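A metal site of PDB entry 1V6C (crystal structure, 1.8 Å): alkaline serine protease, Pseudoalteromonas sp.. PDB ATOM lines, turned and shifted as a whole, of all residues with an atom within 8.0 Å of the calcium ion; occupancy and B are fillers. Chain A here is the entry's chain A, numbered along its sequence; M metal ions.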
ATOM      1  N   ALA A   1      -8.893  16.306 -27.876  1.00  0.00           N
ATOM      2  CA  ALA A   1     -10.166  17.073 -27.797  1.00  0.00           C
ATOM      3  C   ALA A   1     -10.022  18.193 -26.772  1.00  0.00           C
ATOM      4  O   ALA A   1      -9.460  17.994 -25.698  1.00  0.00           O
ATOM      5  CB  ALA A   1     -11.312  16.142 -27.398  1.00  0.00           C
ATOM      6  N   GLU A   2     -10.538  19.362 -27.111  1.00  0.00           N
ATOM      7  CA  GLU A   2     -10.466  20.515 -26.230  1.00  0.00           C
ATOM      8  C   GLU A   2     -11.861  21.005 -25.874  1.00  0.00           C
ATOM      9  O   GLU A   2     -12.710  21.186 -26.743  1.00  0.00           O
ATOM     10  CB  GLU A   2      -9.675  21.626 -26.917  1.00  0.00           C
ATOM     11  CG  GLU A   2      -9.498  22.897 -26.115  1.00  0.00           C
ATOM     12  CD  GLU A   2      -8.501  23.822 -26.756  1.00  0.00           C
ATOM     13  OE1 GLU A   2      -7.361  23.929 -26.246  1.00  0.00           O
ATOM     14  OE2 GLU A   2      -8.844  24.425 -27.796  1.00  0.00           O
ATOM     15  N   THR A   3     -12.088  21.230 -24.578  1.00  0.00           N
ATOM     16  CA  THR A   3     -13.391  21.682 -24.114  1.00  0.00           C
ATOM     17  C   THR A   3     -13.396  23.144 -23.716  1.00  0.00           C
ATOM     18  O   THR A   3     -12.393  23.691 -23.244  1.00  0.00           O
ATOM     19  CB  THR A   3     -13.849  20.830 -22.906  1.00  0.00           C
ATOM     20  OG1 THR A   3     -13.960  19.462 -23.305  1.00  0.00           O
ATOM     21  CG2 THR A   3     -15.191  21.303 -22.380  1.00  0.00           C
ATOM     22  N   HIS A  37       2.742  22.455 -17.259  1.00  0.00           N
ATOM     23  CA  HIS A  37       1.452  22.043 -17.802  1.00  0.00           C
ATOM     24  C   HIS A  37       1.339  22.341 -19.292  1.00  0.00           C
ATOM     25  O   HIS A  37       1.680  23.434 -19.732  1.00  0.00           O
ATOM     26  CB  HIS A  37       0.336  22.768 -17.054  1.00  0.00           C
ATOM     27  CG  HIS A  37      -1.024  22.184 -17.293  1.00  0.00           C
ATOM     28  ND1 HIS A  37      -1.770  21.611 -16.283  1.00  0.00           N
ATOM     29  CD2 HIS A  37      -1.759  22.062 -18.412  1.00  0.00           C
ATOM     30  CE1 HIS A  37      -2.911  21.153 -16.780  1.00  0.00           C
ATOM     31  NE2 HIS A  37      -2.928  21.414 -18.081  1.00  0.00           N
ATOM     32  N   ASN A  38       0.851  21.375 -20.065  1.00  0.00           N
ATOM     33  CA  ASN A  38       0.709  21.564 -21.515  1.00  0.00           C
ATOM     34  C   ASN A  38      -0.150  22.762 -21.897  1.00  0.00           C
ATOM     35  O   ASN A  38       0.108  23.410 -22.915  1.00  0.00           O
ATOM     36  CB  ASN A  38       0.118  20.304 -22.172  1.00  0.00           C
ATOM     37  CG  ASN A  38       1.072  19.128 -22.156  1.00  0.00           C
ATOM     38  OD1 ASN A  38       2.269  19.290 -21.936  1.00  0.00           O
ATOM     39  ND2 ASN A  38       0.539  17.935 -22.406  1.00  0.00           N
ATOM     40  N   ASP A  39      -1.169  23.058 -21.109  1.00  0.00           N
ATOM     41  CA  ASP A  39      -2.060  24.176 -21.416  1.00  0.00           C
ATOM     42  C   ASP A  39      -1.572  25.523 -20.866  1.00  0.00           C
ATOM     43  O   ASP A  39      -2.253  26.529 -21.015  1.00  0.00           O
ATOM     44  CB  ASP A  39      -3.470  23.880 -20.903  1.00  0.00           C
ATOM     45  CG  ASP A  39      -4.435  23.516 -22.020  1.00  0.00           C
ATOM     46  OD1 ASP A  39      -3.976  23.184 -23.134  1.00  0.00           O
ATOM     47  OD2 ASP A  39      -5.662  23.554 -21.792  1.00  0.00           O
ATOM     48  N   LEU A  40      -0.383  25.540 -20.276  1.00  0.00           N
ATOM     49  CA  LEU A  40       0.168  26.779 -19.708  1.00  0.00           C
ATOM     50  C   LEU A  40       1.633  27.068 -20.037  1.00  0.00           C
ATOM     51  O   LEU A  40       2.076  28.218 -19.971  1.00  0.00           O
ATOM     52  CB  LEU A  40       0.008  26.763 -18.184  1.00  0.00           C
ATOM     53  CG  LEU A  40      -1.411  26.764 -17.618  1.00  0.00           C
ATOM     54  CD1 LEU A  40      -1.337  26.549 -16.115  1.00  0.00           C
ATOM     55  CD2 LEU A  40      -2.108  28.085 -17.950  1.00  0.00           C
ATOM     56  N   ALA A  74      -5.872  32.170 -19.053  1.00  0.00           N
ATOM     57  CA  ALA A  74      -5.138  31.906 -20.281  1.00  0.00           C
ATOM     58  C   ALA A  74      -4.818  30.470 -20.677  1.00  0.00           C
ATOM     59  O   ALA A  74      -3.786  30.229 -21.317  1.00  0.00           O
ATOM     60  CB  ALA A  74      -3.847  32.719 -20.263  1.00  0.00           C
ATOM     61  N   ALA A  75      -5.663  29.500 -20.326  1.00  0.00           N
ATOM     62  CA  ALA A  75      -5.389  28.124 -20.748  1.00  0.00           C
ATOM     63  C   ALA A  75      -5.244  28.198 -22.272  1.00  0.00           C
ATOM     64  O   ALA A  75      -6.086  28.793 -22.954  1.00  0.00           O
ATOM     65  CB  ALA A  75      -6.544  27.212 -20.364  1.00  0.00           C
ATOM     66  N   ILE A  76      -4.192  27.592 -22.801  1.00  0.00           N
ATOM     67  CA  ILE A  76      -3.894  27.642 -24.230  1.00  0.00           C
ATOM     68  C   ILE A  76      -4.801  26.850 -25.189  1.00  0.00           C
ATOM     69  O   ILE A  76      -5.164  25.700 -24.923  1.00  0.00           O
ATOM     70  CB  ILE A  76      -2.423  27.232 -24.482  1.00  0.00           C
ATOM     71  CG1 ILE A  76      -1.504  28.171 -23.701  1.00  0.00           C
ATOM     72  CG2 ILE A  76      -2.089  27.291 -25.982  1.00  0.00           C
ATOM     73  CD1 ILE A  76      -0.041  27.729 -23.659  1.00  0.00           C
ATOM     74  N   ALA A  77      -5.134  27.486 -26.310  1.00  0.00           N
ATOM     75  CA  ALA A  77      -5.950  26.850 -27.340  1.00  0.00           C
ATOM     76  C   ALA A  77      -5.020  25.904 -28.093  1.00  0.00           C
ATOM     77  O   ALA A  77      -4.045  26.360 -28.712  1.00  0.00           O
ATOM     78  CB  ALA A  77      -6.527  27.911 -28.284  1.00  0.00           C
ATOM     79  N   ASN A  78      -5.304  24.608 -28.042  1.00  0.00           N
ATOM     80  CA  ASN A  78      -4.447  23.624 -28.701  1.00  0.00           C
ATOM     81  C   ASN A  78      -5.073  22.243 -28.863  1.00  0.00           C
ATOM     82  O   ASN A  78      -4.363  21.234 -28.857  1.00  0.00           O
ATOM     83  CB  ASN A  78      -3.150  23.492 -27.918  1.00  0.00           C
ATOM     84  CG  ASN A  78      -3.400  23.228 -26.435  1.00  0.00           C
ATOM     85  OD1 ASN A  78      -4.510  22.861 -26.041  1.00  0.00           O
ATOM     86  ND2 ASN A  78      -2.364  23.392 -25.622  1.00  0.00           N
ATOM     87  N   ASN A  79      -6.395  22.174 -28.998  1.00  0.00           N
ATOM     88  CA  ASN A  79      -7.059  20.877 -29.191  1.00  0.00           C
ATOM     89  C   ASN A  79      -6.884  19.871 -28.036  1.00  0.00           C
ATOM     90  O   ASN A  79      -7.035  18.660 -28.233  1.00  0.00           O
ATOM     91  CB  ASN A  79      -6.596  20.236 -30.498  1.00  0.00           C
ATOM     92  CG  ASN A  79      -7.431  19.020 -30.888  1.00  0.00           C
ATOM     93  OD1 ASN A  79      -8.647  19.121 -31.063  1.00  0.00           O
ATOM     94  ND2 ASN A  79      -6.782  17.872 -31.031  1.00  0.00           N
ATOM     95  N   GLU A  80      -6.555  20.367 -26.848  1.00  0.00           N
ATOM     96  CA  GLU A  80      -6.416  19.487 -25.684  1.00  0.00           C
ATOM     97  C   GLU A  80      -6.751  20.303 -24.439  1.00  0.00           C
ATOM     98  O   GLU A  80      -6.573  21.521 -24.429  1.00  0.00           O
ATOM     99  CB  GLU A  80      -4.981  18.935 -25.579  1.00  0.00           C
ATOM    100  CG  GLU A  80      -4.081  19.623 -24.557  1.00  0.00           C
ATOM    101  CD  GLU A  80      -2.678  19.032 -24.528  1.00  0.00           C
ATOM    102  OE1 GLU A  80      -1.940  19.192 -25.524  1.00  0.00           O
ATOM    103  OE2 GLU A  80      -2.314  18.403 -23.515  1.00  0.00           O
ATOM    104  N   GLY A  81      -7.253  19.635 -23.410  1.00  0.00           N
ATOM    105  CA  GLY A  81      -7.608  20.343 -22.187  1.00  0.00           C
ATOM    106  C   GLY A  81      -8.735  21.352 -22.343  1.00  0.00           C
ATOM    107  O   GLY A  81      -9.813  21.012 -22.817  1.00  0.00           O
ATOM    108  N   VAL A  82      -8.473  22.591 -21.952  1.00  0.00           N
ATOM    109  CA  VAL A  82      -9.482  23.640 -22.045  1.00  0.00           C
ATOM    110  C   VAL A  82      -8.909  24.903 -22.676  1.00  0.00           C
ATOM    111  O   VAL A  82      -7.832  24.869 -23.280  1.00  0.00           O
ATOM    112  CB  VAL A  82     -10.014  23.996 -20.627  1.00  0.00           C
ATOM    113  CG1 VAL A  82     -10.603  22.760 -19.956  1.00  0.00           C
ATOM    114  CG2 VAL A  82      -8.876  24.546 -19.773  1.00  0.00           C
ATOM    115  N   VAL A  83      -9.646  25.998 -22.561  1.00  0.00           N
ATOM    116  CA  VAL A  83      -9.236  27.283 -23.090  1.00  0.00           C
ATOM    117  C   VAL A  83      -9.608  28.367 -22.078  1.00  0.00           C
ATOM    118  O   VAL A  83     -10.650  28.276 -21.415  1.00  0.00           O
ATOM    119  CB  VAL A  83      -9.918  27.606 -24.455  1.00  0.00           C
ATOM    120  CG1 VAL A  83      -9.377  26.698 -25.542  1.00  0.00           C
ATOM    121  CG2 VAL A  83     -11.421  27.441 -24.332  1.00  0.00           C
ATOM    122  N   GLY A  84      -8.756  29.371 -21.950  1.00  0.00           N
ATOM    123  CA  GLY A  84      -9.012  30.474 -21.036  1.00  0.00           C
ATOM    124  C   GLY A  84      -9.553  31.678 -21.787  1.00  0.00           C
ATOM    125  O   GLY A  84      -9.777  31.599 -22.996  1.00  0.00           O
ATOM    126  N   PRO A  87      -6.665  32.612 -24.801  1.00  0.00           N
ATOM    127  CA  PRO A  87      -5.971  31.361 -25.091  1.00  0.00           C
ATOM    128  C   PRO A  87      -4.989  31.282 -26.264  1.00  0.00           C
ATOM    129  O   PRO A  87      -4.403  30.221 -26.483  1.00  0.00           O
ATOM    130  CB  PRO A  87      -7.129  30.405 -25.297  1.00  0.00           C
ATOM    131  CG  PRO A  87      -8.052  31.257 -26.145  1.00  0.00           C
ATOM    132  CD  PRO A  87      -7.978  32.636 -25.460  1.00  0.00           C
ATOM    133  N   THR A 208      -7.241  24.227 -15.467  1.00  0.00           N
ATOM    134  CA  THR A 208      -5.978  23.530 -15.274  1.00  0.00           C
ATOM    135  C   THR A 208      -5.574  23.488 -13.799  1.00  0.00           C
ATOM    136  O   THR A 208      -5.865  24.417 -13.046  1.00  0.00           O
ATOM    137  CB  THR A 208      -4.854  24.259 -16.021  1.00  0.00           C
ATOM    138  OG1 THR A 208      -4.859  25.649 -15.655  1.00  0.00           O
ATOM    139  CG2 THR A 208      -5.023  24.132 -17.534  1.00  0.00           C
ATOM    140  N   TYR A 362      -6.665  18.520 -14.881  1.00  0.00           N
ATOM    141  CA  TYR A 362      -7.724  19.525 -14.858  1.00  0.00           C
ATOM    142  C   TYR A 362      -8.674  19.138 -13.725  1.00  0.00           C
ATOM    143  O   TYR A 362      -8.681  17.994 -13.282  1.00  0.00           O
ATOM    144  CB  TYR A 362      -8.498  19.527 -16.183  1.00  0.00           C
ATOM    145  CG  TYR A 362      -7.611  19.723 -17.393  1.00  0.00           C
ATOM    146  CD1 TYR A 362      -7.308  20.992 -17.864  1.00  0.00           C
ATOM    147  CD2 TYR A 362      -7.004  18.626 -18.010  1.00  0.00           C
ATOM    148  CE1 TYR A 362      -6.424  21.177 -18.931  1.00  0.00           C
ATOM    149  CE2 TYR A 362      -6.111  18.792 -19.063  1.00  0.00           C
ATOM    150  CZ  TYR A 362      -5.819  20.069 -19.517  1.00  0.00           C
ATOM    151  OH  TYR A 362      -4.929  20.245 -20.547  1.00  0.00           O
HETATM  152 CA    CA M   1      -6.021  23.666 -24.313  1.00  0.00          CA
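Within 4 Å of the calcium ion: Glu 2, Asp 39, Ile 76, Asn 78, Glu 80 and Val 82.
Along chain A the residues within 4 Å of the calcium ion span positions 2 to 82.
The nearest printed residue that does not touch the calcium ion is Gly 81 (4.1 Å).
The calcium ion is bound by the backbone carbonyl oxygen (O) of Glu 80 (2.2 Å), the backbone carbonyl oxygen (O) of Ile 76 (2.3 Å), the side-chain carboxylate (OE1) of Glu 2 (2.4 Å), the backbone carbonyl oxygen (O) of Val 82 (2.4 Å), the side-chain carboxylate (OD1) of Asp 39 (2.4 Å), the side-chain amide oxygen (OD1) of Asn 78 (2.4 Å) and the side-chain carboxylate (OD2) of Asp 39 (2.5 Å).
ND2 of Asn 38 sits at hydrogen-bond distance from OE2 of Glu 80 (3.1 Å).
The side-chain carboxylate of Glu 2 lies close to the backbone NH of Asn 79 (3.4 Å).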
